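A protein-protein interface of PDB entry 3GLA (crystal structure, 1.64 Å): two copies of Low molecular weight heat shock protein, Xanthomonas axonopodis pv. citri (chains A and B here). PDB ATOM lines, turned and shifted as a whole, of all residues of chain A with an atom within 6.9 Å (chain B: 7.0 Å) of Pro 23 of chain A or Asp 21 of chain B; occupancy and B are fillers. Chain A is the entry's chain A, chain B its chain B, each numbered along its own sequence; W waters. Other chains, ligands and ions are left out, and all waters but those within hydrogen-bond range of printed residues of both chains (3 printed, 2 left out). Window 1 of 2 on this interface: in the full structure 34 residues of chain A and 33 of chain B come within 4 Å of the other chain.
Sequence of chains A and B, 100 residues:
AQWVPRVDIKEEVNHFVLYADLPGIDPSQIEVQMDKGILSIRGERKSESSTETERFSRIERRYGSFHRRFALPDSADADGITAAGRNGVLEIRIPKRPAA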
ATOM      1  N   TRP A   3       4.459  -4.998   0.410  1.00  0.00           N
ATOM      2  CA  TRP A   3       5.082  -3.835  -0.217  1.00  0.00           C
ATOM      3  C   TRP A   3       5.868  -4.303  -1.438  1.00  0.00           C
ATOM      4  O   TRP A   3       6.027  -5.480  -1.607  1.00  0.00           O
ATOM      5  CB  TRP A   3       6.049  -3.116   0.605  1.00  0.00           C
ATOM      6  CG  TRP A   3       7.267  -3.790   0.920  1.00  0.00           C
ATOM      7  CD1 TRP A   3       7.345  -4.952   1.649  1.00  0.00           C
ATOM      8  CD2 TRP A   3       8.670  -3.375   0.696  1.00  0.00           C
ATOM      9  NE1 TRP A   3       8.689  -5.286   1.956  1.00  0.00           N
ATOM     10  CE2 TRP A   3       9.538  -4.356   1.369  1.00  0.00           C
ATOM     11  CE3 TRP A   3       9.291  -2.227   0.074  1.00  0.00           C
ATOM     12  CZ2 TRP A   3      10.937  -4.299   1.376  1.00  0.00           C
ATOM     13  CZ3 TRP A   3      10.667  -2.195   0.124  1.00  0.00           C
ATOM     14  CH2 TRP A   3      11.504  -3.156   0.748  1.00  0.00           C
ATOM     15  N   PRO A   5       9.018  -3.653  -3.591  1.00  0.00           N
ATOM     16  CA  PRO A   5      10.290  -2.967  -3.704  1.00  0.00           C
ATOM     17  C   PRO A   5      10.539  -2.652  -5.170  1.00  0.00           C
ATOM     18  O   PRO A   5      10.091  -3.353  -6.061  1.00  0.00           O
ATOM     19  CB  PRO A   5      11.261  -4.093  -3.362  1.00  0.00           C
ATOM     20  CG  PRO A   5      10.478  -5.043  -2.502  1.00  0.00           C
ATOM     21  CD  PRO A   5       9.016  -4.892  -2.797  1.00  0.00           C
ATOM     22  N   ALA A  20      17.520  -4.584  -7.194  1.00  0.00           N
ATOM     23  CA  ALA A  20      16.266  -4.507  -6.393  1.00  0.00           C
ATOM     24  C   ALA A  20      16.674  -3.670  -5.186  1.00  0.00           C
ATOM     25  O   ALA A  20      17.651  -3.889  -4.441  1.00  0.00           O
ATOM     26  CB  ALA A  20      15.864  -5.849  -5.928  1.00  0.00           C
ATOM     27  N   ASP A  21      15.902  -2.627  -4.940  1.00  0.00           N
ATOM     28  CA  ASP A  21      16.129  -1.841  -3.708  1.00  0.00           C
ATOM     29  C   ASP A  21      15.405  -2.520  -2.560  1.00  0.00           C
ATOM     30  O   ASP A  21      14.184  -2.456  -2.399  1.00  0.00           O
ATOM     31  CB  ASP A  21      15.472  -0.475  -3.871  1.00  0.00           C
ATOM     32  CG  ASP A  21      16.275   0.475  -4.725  1.00  0.00           C
ATOM     33  OD1 ASP A  21      17.450   0.191  -4.863  1.00  0.00           O
ATOM     34  OD2 ASP A  21      15.786   1.603  -4.923  1.00  0.00           O
ATOM     35  N   LEU A  22      16.225  -3.139  -1.714  1.00  0.00           N
ATOM     36  CA  LEU A  22      15.689  -3.906  -0.579  1.00  0.00           C
ATOM     37  C   LEU A  22      16.433  -3.454   0.657  1.00  0.00           C
ATOM     38  O   LEU A  22      17.185  -4.232   1.287  1.00  0.00           O
ATOM     39  CB  LEU A  22      16.005  -5.406  -0.852  1.00  0.00           C
ATOM     40  CG  LEU A  22      15.111  -5.912  -2.017  1.00  0.00           C
ATOM     41  CD1 LEU A  22      15.524  -7.266  -2.502  1.00  0.00           C
ATOM     42  CD2 LEU A  22      13.648  -5.916  -1.622  1.00  0.00           C
ATOM     43  N   PRO A  23      16.295  -2.193   1.015  1.00  0.00           N
ATOM     44  CA  PRO A  23      17.001  -1.746   2.177  1.00  0.00           C
ATOM     45  C   PRO A  23      16.490  -2.432   3.422  1.00  0.00           C
ATOM     46  O   PRO A  23      15.341  -2.797   3.544  1.00  0.00           O
ATOM     47  CB  PRO A  23      16.592  -0.282   2.271  1.00  0.00           C
ATOM     48  CG  PRO A  23      15.242  -0.183   1.541  1.00  0.00           C
ATOM     49  CD  PRO A  23      15.484  -1.157   0.360  1.00  0.00           C
ATOM     50  N   GLY A  24      17.443  -2.686   4.303  1.00  0.00           N
ATOM     51  CA  GLY A  24      17.047  -3.074   5.649  1.00  0.00           C
ATOM     52  C   GLY A  24      16.869  -4.562   5.754  1.00  0.00           C
ATOM     53  O   GLY A  24      16.153  -5.014   6.666  1.00  0.00           O
ATOM     54  N   ILE A  25      17.375  -5.288   4.767  1.00  0.00           N
ATOM     55  CA  ILE A  25      17.255  -6.764   4.762  1.00  0.00           C
ATOM     56  C   ILE A  25      18.585  -7.293   4.399  1.00  0.00           C
ATOM     57  O   ILE A  25      19.300  -6.807   3.588  1.00  0.00           O
ATOM     58  CB  ILE A  25      16.221  -7.340   3.777  1.00  0.00           C
ATOM     59  CG1 ILE A  25      14.948  -6.658   3.850  1.00  0.00           C
ATOM     60  CG2 ILE A  25      15.912  -8.860   4.082  1.00  0.00           C
ATOM     61  CD1 ILE A  25      14.370  -6.706   2.506  1.00  0.00           C
ATOM     62  N   ASP A  26      19.094  -8.302   5.177  1.00  0.00           N
ATOM     63  CA  ASP A  26      20.351  -8.893   4.782  1.00  0.00           C
ATOM     64  C   ASP A  26      20.157  -9.713   3.512  1.00  0.00           C
ATOM     65  O   ASP A  26      19.090 -10.331   3.455  1.00  0.00           O
ATOM     66  CB  ASP A  26      20.806  -9.942   5.813  1.00  0.00           C
ATOM     67  CG  ASP A  26      21.515  -9.314   7.004  1.00  0.00           C
ATOM     68  OD1 ASP A  26      22.201  -8.231   6.863  1.00  0.00           O
ATOM     69  OD2 ASP A  26      21.392  -9.968   8.077  1.00  0.00           O
ATOM     70  N   ARG A  45      10.721  -8.000   4.933  1.00  0.00           N
ATOM     71  CA  ARG A  45      11.515  -7.035   5.564  1.00  0.00           C
ATOM     72  C   ARG A  45      10.857  -6.652   6.879  1.00  0.00           C
ATOM     73  O   ARG A  45       9.672  -6.446   6.924  1.00  0.00           O
ATOM     74  CB  ARG A  45      11.432  -5.724   4.662  1.00  0.00           C
ATOM     75  CG  ARG A  45      12.178  -4.690   5.348  1.00  0.00           C
ATOM     76  CD  ARG A  45      12.025  -3.271   4.611  1.00  0.00           C
ATOM     77  NE  ARG A  45      12.775  -2.334   5.358  1.00  0.00           N
ATOM     78  CZ  ARG A  45      13.055  -1.088   4.916  1.00  0.00           C
ATOM     79  NH1 ARG A  45      12.315  -0.610   3.962  1.00  0.00           N
ATOM     80  NH2 ARG A  45      13.986  -0.360   5.552  1.00  0.00           N
ATOM     81  N   LYS A  46      11.679  -6.588   7.898  1.00  0.00           N
ATOM     82  CA  LYS A  46      11.211  -6.187   9.230  1.00  0.00           C
ATOM     83  C   LYS A  46      11.494  -4.703   9.309  1.00  0.00           C
ATOM     84  O   LYS A  46      12.416  -4.209   8.637  1.00  0.00           O
ATOM     85  CB  LYS A  46      12.126  -6.901  10.248  1.00  0.00           C
ATOM     86  CG  LYS A  46      12.110  -8.398  10.020  1.00  0.00           C
ATOM     87  CD  LYS A  46      10.721  -8.833  10.363  1.00  0.00           C
ATOM     88  CE  LYS A  46      10.734 -10.413  10.404  1.00  0.00           C
ATOM     89  NZ  LYS A  46       9.345 -10.854  10.199  1.00  0.00           N
ATOM     90  N   GLU A  48      11.832  -1.279  12.196  1.00  0.00           N
ATOM     91  CA  GLU A  48      11.785  -0.793  13.538  1.00  0.00           C
ATOM     92  C   GLU A  48      10.455  -0.224  13.849  1.00  0.00           C
ATOM     93  O   GLU A  48      10.083  -0.175  15.017  1.00  0.00           O
ATOM     94  CB  GLU A  48      12.853   0.248  13.735  1.00  0.00           C
ATOM     95  CG  GLU A  48      14.288  -0.329  13.561  1.00  0.00           C
ATOM     96  CD  GLU A  48      14.782  -0.348  12.040  1.00  0.00           C
ATOM     97  OE1 GLU A  48      13.933  -0.134  11.125  1.00  0.00           O
ATOM     98  OE2 GLU A  48      16.008  -0.518  11.784  1.00  0.00           O
ATOM     99  N   GLU A  60       7.285   6.174   7.211  1.00  0.00           N
ATOM    100  CA  GLU A  60       7.189   6.234   5.787  1.00  0.00           C
ATOM    101  C   GLU A  60       7.730   4.945   5.187  1.00  0.00           C
ATOM    102  O   GLU A  60       7.425   4.669   4.035  1.00  0.00           O
ATOM    103  CB  GLU A  60       8.014   7.306   5.088  1.00  0.00           C
ATOM    104  CG  GLU A  60       7.562   8.717   5.630  1.00  0.00           C
ATOM    105  CD  GLU A  60       8.472   9.787   5.212  1.00  0.00           C
ATOM    106  OE1 GLU A  60       9.500   9.498   4.623  1.00  0.00           O
ATOM    107  OE2 GLU A  60       8.099  10.975   5.408  1.00  0.00           O
ATOM    108  N   ARG A  61       8.543   4.226   5.890  1.00  0.00           N
ATOM    109  CA  ARG A  61       9.214   3.128   5.219  1.00  0.00           C
ATOM    110  C   ARG A  61       8.359   1.931   5.152  1.00  0.00           C
ATOM    111  O   ARG A  61       7.707   1.553   6.113  1.00  0.00           O
ATOM    112  CB  ARG A  61      10.516   2.769   5.967  1.00  0.00           C
ATOM    113  CG  ARG A  61      11.432   4.019   5.944  1.00  0.00           C
ATOM    114  CD  ARG A  61      12.796   3.683   6.531  1.00  0.00           C
ATOM    115  NE  ARG A  61      12.649   2.934   7.633  1.00  0.00           N
ATOM    116  CZ  ARG A  61      13.361   2.064   8.322  1.00  0.00           C
ATOM    117  NH1 ARG A  61      14.463   1.387   8.014  1.00  0.00           N
ATOM    118  NH2 ARG A  61      12.763   1.793   9.416  1.00  0.00           N
ATOM    119  N   ARG A  62       8.326   1.349   3.940  1.00  0.00           N
ATOM    120  CA  ARG A  62       7.441   0.193   3.798  1.00  0.00           C
ATOM    121  C   ARG A  62       8.191  -1.058   4.162  1.00  0.00           C
ATOM    122  O   ARG A  62       9.411  -1.161   3.992  1.00  0.00           O
ATOM    123  CB  ARG A  62       7.073   0.079   2.300  1.00  0.00           C
ATOM    124  CG  ARG A  62       6.134   1.360   1.954  1.00  0.00           C
ATOM    125  CD  ARG A  62       6.019   1.324   0.428  1.00  0.00           C
ATOM    126  NE  ARG A  62       5.081   2.362  -0.066  1.00  0.00           N
ATOM    127  CZ  ARG A  62       5.168   2.980  -1.239  1.00  0.00           C
ATOM    128  NH1 ARG A  62       6.182   2.782  -2.141  1.00  0.00           N
ATOM    129  NH2 ARG A  62       4.212   3.857  -1.514  1.00  0.00           N
ATOM    130  N   ASN A  87      24.661  -2.323   0.406  1.00  0.00           N
ATOM    131  CA  ASN A  87      23.895  -1.111   0.793  1.00  0.00           C
ATOM    132  C   ASN A  87      22.438  -1.261   0.454  1.00  0.00           C
ATOM    133  O   ASN A  87      21.840  -0.276   0.034  1.00  0.00           O
ATOM    134  CB  ASN A  87      24.438   0.162   0.200  1.00  0.00           C
ATOM    135  CG  ASN A  87      25.858   0.434   0.642  1.00  0.00           C
ATOM    136  OD1 ASN A  87      26.736   0.700  -0.198  1.00  0.00           O
ATOM    137  ND2 ASN A  87      26.084   0.345   1.884  1.00  0.00           N
ATOM    138  N   GLY A  88      21.932  -2.463   0.602  1.00  0.00           N
ATOM    139  CA  GLY A  88      20.448  -2.623   0.408  1.00  0.00           C
ATOM    140  C   GLY A  88      20.024  -2.712  -1.026  1.00  0.00           C
ATOM    141  O   GLY A  88      18.843  -2.841  -1.226  1.00  0.00           O
ATOM    142  N   VAL A  89      20.968  -2.741  -1.945  1.00  0.00           N
ATOM    143  CA  VAL A  89      20.574  -3.036  -3.319  1.00  0.00           C
ATOM    144  C   VAL A  89      20.997  -4.436  -3.583  1.00  0.00           C
ATOM    145  O   VAL A  89      22.212  -4.719  -3.526  1.00  0.00           O
ATOM    146  CB  VAL A  89      21.183  -2.107  -4.321  1.00  0.00           C
ATOM    147  CG1 VAL A  89      20.898  -2.546  -5.746  1.00  0.00           C
ATOM    148  CG2 VAL A  89      20.698  -0.688  -4.078  1.00  0.00           C
ATOM    149  N   TRP B   3      14.125  11.731  -5.906  1.00  0.00           N
ATOM    150  CA  TRP B   3      14.159  10.618  -5.090  1.00  0.00           C
ATOM    151  C   TRP B   3      13.773  11.338  -3.740  1.00  0.00           C
ATOM    152  O   TRP B   3      14.387  12.355  -3.341  1.00  0.00           O
ATOM    153  CB  TRP B   3      15.543  10.048  -5.017  1.00  0.00           C
ATOM    154  CG  TRP B   3      15.777   8.919  -4.075  1.00  0.00           C
ATOM    155  CD1 TRP B   3      14.829   7.980  -3.546  1.00  0.00           C
ATOM    156  CD2 TRP B   3      17.033   8.500  -3.644  1.00  0.00           C
ATOM    157  NE1 TRP B   3      15.497   7.087  -2.779  1.00  0.00           N
ATOM    158  CE2 TRP B   3      16.829   7.308  -2.848  1.00  0.00           C
ATOM    159  CE3 TRP B   3      18.284   8.954  -3.846  1.00  0.00           C
ATOM    160  CZ2 TRP B   3      17.798   6.670  -2.245  1.00  0.00           C
ATOM    161  CZ3 TRP B   3      19.320   8.261  -3.204  1.00  0.00           C
ATOM    162  CH2 TRP B   3      19.061   7.124  -2.423  1.00  0.00           C
ATOM    163  N   VAL B   4      12.790  10.779  -3.052  1.00  0.00           N
ATOM    164  CA  VAL B   4      12.490  11.209  -1.705  1.00  0.00           C
ATOM    165  C   VAL B   4      12.603   9.921  -0.882  1.00  0.00           C
ATOM    166  O   VAL B   4      11.671   9.169  -0.756  1.00  0.00           O
ATOM    167  CB  VAL B   4      11.054  11.728  -1.660  1.00  0.00           C
ATOM    168  CG1 VAL B   4      10.729  12.158  -0.268  1.00  0.00           C
ATOM    169  CG2 VAL B   4      10.924  12.979  -2.571  1.00  0.00           C
ATOM    170  N   PRO B   5      13.752   9.701  -0.283  1.00  0.00           N
ATOM    171  CA  PRO B   5      13.987   8.483   0.429  1.00  0.00           C
ATOM    172  C   PRO B   5      13.083   8.476   1.655  1.00  0.00           C
ATOM    173  O   PRO B   5      12.997   9.428   2.358  1.00  0.00           O
ATOM    174  CB  PRO B   5      15.452   8.556   0.886  1.00  0.00           C
ATOM    175  CG  PRO B   5      15.956   9.760   0.285  1.00  0.00           C
ATOM    176  CD  PRO B   5      14.956  10.524  -0.442  1.00  0.00           C
ATOM    177  N   ARG B   6      12.468   7.350   1.896  1.00  0.00           N
ATOM    178  CA  ARG B   6      11.532   7.257   3.022  1.00  0.00           C
ATOM    179  C   ARG B   6      12.198   7.135   4.339  1.00  0.00           C
ATOM    180  O   ARG B   6      13.255   6.525   4.442  1.00  0.00           O
ATOM    181  CB  ARG B   6      10.665   6.008   2.813  1.00  0.00           C
ATOM    182  CG  ARG B   6       9.674   6.331   1.610  1.00  0.00           C
ATOM    183  CD  ARG B   6       8.991   5.007   1.230  1.00  0.00           C
ATOM    184  NE  ARG B   6       8.004   5.421   0.258  1.00  0.00           N
ATOM    185  CZ  ARG B   6       6.768   5.757   0.518  1.00  0.00           C
ATOM    186  NH1 ARG B   6       6.227   5.718   1.681  1.00  0.00           N
ATOM    187  NH2 ARG B   6       6.051   6.158  -0.554  1.00  0.00           N
ATOM    188  N   VAL B   7      11.628   7.764   5.345  1.00  0.00           N
ATOM    189  CA  VAL B   7      12.264   7.854   6.673  1.00  0.00           C
ATOM    190  C   VAL B   7      11.194   7.537   7.710  1.00  0.00           C
ATOM    191  O   VAL B   7       9.974   7.855   7.532  1.00  0.00           O
ATOM    192  CB  VAL B   7      12.637   9.290   6.837  1.00  0.00           C
ATOM    193  CG1 VAL B   7      12.908   9.628   8.226  1.00  0.00           C
ATOM    194  CG2 VAL B   7      13.855   9.562   5.898  1.00  0.00           C
ATOM    195  N   ASP B   8      11.604   6.846   8.689  1.00  0.00           N
ATOM    196  CA  ASP B   8      10.735   6.788   9.893  1.00  0.00           C
ATOM    197  C   ASP B   8      11.442   7.541  10.978  1.00  0.00           C
ATOM    198  O   ASP B   8      12.705   7.561  11.040  1.00  0.00           O
ATOM    199  CB  ASP B   8      10.638   5.355  10.386  1.00  0.00           C
ATOM    200  CG  ASP B   8       9.968   4.440   9.401  1.00  0.00           C
ATOM    201  OD1 ASP B   8       9.302   4.904   8.508  1.00  0.00           O
ATOM    202  OD2 ASP B   8      10.217   3.206   9.575  1.00  0.00           O
ATOM    203  N   LEU B  18      16.160   8.432  13.571  1.00  0.00           N
ATOM    204  CA  LEU B  18      15.604   8.525  12.239  1.00  0.00           C
ATOM    205  C   LEU B  18      16.152   7.382  11.461  1.00  0.00           C
ATOM    206  O   LEU B  18      17.350   7.069  11.540  1.00  0.00           O
ATOM    207  CB  LEU B  18      16.001   9.810  11.636  1.00  0.00           C
ATOM    208  CG  LEU B  18      15.449  10.092  10.244  1.00  0.00           C
ATOM    209  CD1 LEU B  18      15.263  11.702  10.058  1.00  0.00           C
ATOM    210  CD2 LEU B  18      16.411   9.415   9.143  1.00  0.00           C
ATOM    211  N   TYR B  19      15.269   6.702  10.731  1.00  0.00           N
ATOM    212  CA  TYR B  19      15.743   5.557   9.947  1.00  0.00           C
ATOM    213  C   TYR B  19      15.429   5.935   8.519  1.00  0.00           C
ATOM    214  O   TYR B  19      14.317   6.359   8.219  1.00  0.00           O
ATOM    215  CB  TYR B  19      14.903   4.324  10.253  1.00  0.00           C
ATOM    216  CG  TYR B  19      14.908   3.925  11.694  1.00  0.00           C
ATOM    217  CD1 TYR B  19      15.859   3.064  12.178  1.00  0.00           C
ATOM    218  CD2 TYR B  19      13.923   4.423  12.541  1.00  0.00           C
ATOM    219  CE1 TYR B  19      15.841   2.676  13.556  1.00  0.00           C
ATOM    220  CE2 TYR B  19      13.881   4.047  13.833  1.00  0.00           C
ATOM    221  CZ  TYR B  19      14.831   3.168  14.302  1.00  0.00           C
ATOM    222  OH  TYR B  19      14.765   2.896  15.676  1.00  0.00           O
ATOM    223  N   ALA B  20      16.456   5.929   7.650  1.00  0.00           N
ATOM    224  CA  ALA B  20      16.205   6.370   6.309  1.00  0.00           C
ATOM    225  C   ALA B  20      16.542   5.241   5.368  1.00  0.00           C
ATOM    226  O   ALA B  20      17.601   4.622   5.448  1.00  0.00           O
ATOM    227  CB  ALA B  20      17.101   7.569   6.018  1.00  0.00           C
ATOM    228  N   ASP B  21      15.687   5.023   4.436  1.00  0.00           N
ATOM    229  CA  ASP B  21      15.987   3.996   3.453  1.00  0.00           C
ATOM    230  C   ASP B  21      16.751   4.708   2.340  1.00  0.00           C
ATOM    231  O   ASP B  21      16.209   5.432   1.482  1.00  0.00           O
ATOM    232  CB  ASP B  21      14.662   3.516   2.903  1.00  0.00           C
ATOM    233  CG  ASP B  21      14.085   2.385   3.746  1.00  0.00           C
ATOM    234  OD1 ASP B  21      14.705   2.018   4.735  1.00  0.00           O
ATOM    235  OD2 ASP B  21      12.951   1.996   3.397  1.00  0.00           O
ATOM    236  N   LEU B  22      18.045   4.388   2.353  1.00  0.00           N
ATOM    237  CA  LEU B  22      18.962   4.993   1.366  1.00  0.00           C
ATOM    238  C   LEU B  22      19.711   3.895   0.680  1.00  0.00           C
ATOM    239  O   LEU B  22      20.935   3.865   0.713  1.00  0.00           O
ATOM    240  CB  LEU B  22      19.905   5.967   2.134  1.00  0.00           C
ATOM    241  CG  LEU B  22      19.047   7.240   2.570  1.00  0.00           C
ATOM    242  CD1 LEU B  22      19.993   7.913   3.586  1.00  0.00           C
ATOM    243  CD2 LEU B  22      18.736   8.042   1.382  1.00  0.00           C
ATOM    244  N   PRO B  23      18.979   3.037  -0.025  1.00  0.00           N
ATOM    245  CA  PRO B  23      19.715   1.922  -0.649  1.00  0.00           C
ATOM    246  C   PRO B  23      20.626   2.425  -1.759  1.00  0.00           C
ATOM    247  O   PRO B  23      20.442   3.448  -2.369  1.00  0.00           O
ATOM    248  CB  PRO B  23      18.595   1.094  -1.239  1.00  0.00           C
ATOM    249  CG  PRO B  23      17.418   2.072  -1.597  1.00  0.00           C
ATOM    250  CD  PRO B  23      17.531   2.992  -0.308  1.00  0.00           C
ATOM    251  N   GLY B  24      21.789   1.784  -1.792  1.00  0.00           N
ATOM    252  CA  GLY B  24      22.644   2.027  -2.954  1.00  0.00           C
ATOM    253  C   GLY B  24      23.623   3.170  -2.712  1.00  0.00           C
ATOM    254  O   GLY B  24      24.203   3.676  -3.704  1.00  0.00           O
ATOM    255  N   ILE B  41      19.123  15.277   5.786  1.00  0.00           N
ATOM    256  CA  ILE B  41      19.899  14.261   5.154  1.00  0.00           C
ATOM    257  C   ILE B  41      20.010  14.614   3.713  1.00  0.00           C
ATOM    258  O   ILE B  41      19.036  15.019   3.101  1.00  0.00           O
ATOM    259  CB  ILE B  41      19.305  12.821   5.296  1.00  0.00           C
ATOM    260  CG1 ILE B  41      17.847  12.779   4.760  1.00  0.00           C
ATOM    261  CG2 ILE B  41      19.368  12.421   6.750  1.00  0.00           C
ATOM    262  CD1 ILE B  41      17.277  11.316   4.664  1.00  0.00           C
ATOM    263  N   ARG B  86      23.326   0.295   7.547  1.00  0.00           N
ATOM    264  CA  ARG B  86      23.476  -1.135   7.303  1.00  0.00           C
ATOM    265  C   ARG B  86      22.397  -1.515   6.323  1.00  0.00           C
ATOM    266  O   ARG B  86      21.236  -1.095   6.448  1.00  0.00           O
ATOM    267  CB  ARG B  86      23.203  -1.862   8.636  1.00  0.00           C
ATOM    268  CG  ARG B  86      23.273  -3.353   8.449  1.00  0.00           C
ATOM    269  CD  ARG B  86      23.174  -3.996   9.869  1.00  0.00           C
ATOM    270  NE  ARG B  86      24.071  -5.135   9.788  1.00  0.00           N
ATOM    271  CZ  ARG B  86      23.661  -6.343   9.401  1.00  0.00           C
ATOM    272  NH1 ARG B  86      22.372  -6.547   9.162  1.00  0.00           N
ATOM    273  NH2 ARG B  86      24.512  -7.345   9.292  1.00  0.00           N
ATOM    274  N   ASN B  87      22.828  -2.226   5.282  1.00  0.00           N
ATOM    275  CA  ASN B  87      21.889  -2.674   4.259  1.00  0.00           C
ATOM    276  C   ASN B  87      21.095  -1.512   3.726  1.00  0.00           C
ATOM    277  O   ASN B  87      19.916  -1.715   3.462  1.00  0.00           O
ATOM    278  CB  ASN B  87      20.975  -3.739   4.819  1.00  0.00           C
ATOM    279  CG  ASN B  87      21.707  -5.040   5.052  1.00  0.00           C
ATOM    280  OD1 ASN B  87      22.581  -5.387   4.289  1.00  0.00           O
ATOM    281  ND2 ASN B  87      21.398  -5.679   6.195  1.00  0.00           N
ATOM    282  N   GLY B  88      21.716  -0.346   3.528  1.00  0.00           N
ATOM    283  CA  GLY B  88      20.982   0.727   2.841  1.00  0.00           C
ATOM    284  C   GLY B  88      20.147   1.520   3.791  1.00  0.00           C
ATOM    285  O   GLY B  88      19.456   2.379   3.294  1.00  0.00           O
ATOM    286  N   VAL B  89      20.078   1.168   5.067  1.00  0.00           N
ATOM    287  CA  VAL B  89      19.278   1.983   5.962  1.00  0.00           C
ATOM    288  C   VAL B  89      20.241   2.757   6.762  1.00  0.00           C
ATOM    289  O   VAL B  89      21.251   2.250   7.319  1.00  0.00           O
ATOM    290  CB  VAL B  89      18.428   1.103   6.931  1.00  0.00           C
ATOM    291  CG1 VAL B  89      17.827   1.987   8.008  1.00  0.00           C
ATOM    292  CG2 VAL B  89      17.400   0.350   6.120  1.00  0.00           C
ATOM    293  N   LEU B  90      19.966   4.021   6.857  1.00  0.00           N
ATOM    294  CA  LEU B  90      20.860   4.846   7.735  1.00  0.00           C
ATOM    295  C   LEU B  90      20.078   5.126   8.974  1.00  0.00           C
ATOM    296  O   LEU B  90      18.908   5.527   8.871  1.00  0.00           O
ATOM    297  CB  LEU B  90      21.136   6.160   7.009  1.00  0.00           C
ATOM    298  CG  LEU B  90      22.080   7.089   7.864  1.00  0.00           C
ATOM    299  CD1 LEU B  90      23.434   6.486   7.903  1.00  0.00           C
ATOM    300  CD2 LEU B  90      22.184   8.440   7.192  1.00  0.00           C
HETATM  301  O   HOH W   1       3.983   4.492   3.925  1.00  0.00           O
HETATM  302  O   HOH W   2       8.643   1.402   8.733  1.00  0.00           O
HETATM  303  O   HOH W   3      22.943  -4.881   1.473  1.00  0.00           O
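The side-chain carboxylate of Asp 8 of chain B lies within hydrogen-bond range of the backbone NH of Glu 60 of chain A, 2.7 Å away.
The guanidinium group of Arg 61 of chain A lies within salt-bridge range of the side-chain carboxylate of Asp 21 of chain B, 3.3 Å away.
OD1 of Asp 21 of chain B lies within salt-bridge range of NH2 of Arg 45 of chain A, at 2.6 Å.
The guanidinium group of Arg 62 of chain A lies close to the guanidinium group of Arg 6 of chain B, 3.1 Å away.
The backbone carbonyl oxygen (O) of Asn 87 of chain A lies close to the backbone NH (N) of Gly 88 of chain B (3.5 Å).
The backbone carbonyl oxygen of Glu 60 of chain A is in hydrogen-bond range of the guanidinium group of Arg 6 of chain B, 2.8 Å away.
The side-chain carboxylate (OD1) of Asp 26 of chain A lies within salt-bridge range of the guanidinium group (NH1) of Arg 86 of chain B (2.9 Å).
The guanidinium group of Arg 61 of chain A lies within salt-bridge range of the side-chain carboxylate of Asp 8 of chain B, at 2.9 Å.
ND2 of Asn 87 of chain B sits at hydrogen-bond distance from OD1 of Asp 26 of chain A (2.8 Å).
The side-chain carboxylate (OE1) of Glu 60 of chain A is in hydrogen-bond range of the backbone NH (N) of Val 7 of chain B.
O of Asn 87 of chain B lies within hydrogen-bond range of N of Gly 24 of chain A.
O of Asn 87 of chain A sits at hydrogen-bond distance from N of Gly 24 of chain B (2.8 Å).
Of the 18 printed residues of chain A, 13 touch a printed residue of chain B.
Printed residues of chain A that touch a printed residue of chain B: Asp 21, Pro 23, Gly 24, Ile 25, Asp 26, Arg 45, Glu 48, Glu 60, Arg 61, Arg 62, Asn 87, Gly 88 and Val 89.
Hydrophobic or aromatic side chains of chain A that line the printed part of chain B: Pro 23 and Val 89.
Among the printed residues, Asp or Glu carboxylates within 4 Å of a Lys or Arg side-chain nitrogen of the other chain: Asp 26 of chain A with Arg 86 of chain B, Arg 45 of chain A with Asp 21 of chain B, Arg 61 of chain A with Asp 8 of chain B and Arg 61 of chain A with Asp 21 of chain B.
N of Leu 22 of chain B is in hydrogen-bond range of O of Gly 88 of chain B (2.6 Å).
OE1 of Glu 48 of chain A is in salt-bridge range of NH2 of Arg 61 of chain A, 2.8 Å away.
10 positions are printed for both chains.
Of the 31 pairs that touch across the chains among the printed residues, 14 have their exchanged pair printed and touching as well.
Water W2 bridges OD2 of Asp 8 of chain B and O of Arg 61 of chain A.
Water W1 bridges NH1 of Arg 6 of chain B and O of Glu 60 of chain A.
Pro 23 of chain B touches Asp 21 of chain A.
Asp 21 of chain B touches Pro 23 of chain A.
Arg 45 of chain A touches Val 89 of chain B.
Arg 61 of chain A touches Val 7 of chain B (CG to N, 3.8 Å).
CZ of Arg 61 of chain A touches CB of Tyr 19 of chain B (3.3 Å).
Pro 5 of chain A touches none of the printed residues of chain B.
Of the printed residues of chain B, Glu 48 of chain A touches Tyr 19 (3.4 Å).
Of the printed residues of chain B, Asn 87 of chain A touches Pro 23, Gly 24, Asn 87 and Gly 88.
Asp 21 of chain B touches just these residues of chain A: Pro 23 (3.6 Å), Arg 45 (2.6 Å) and Arg 61 (3.1 Å).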
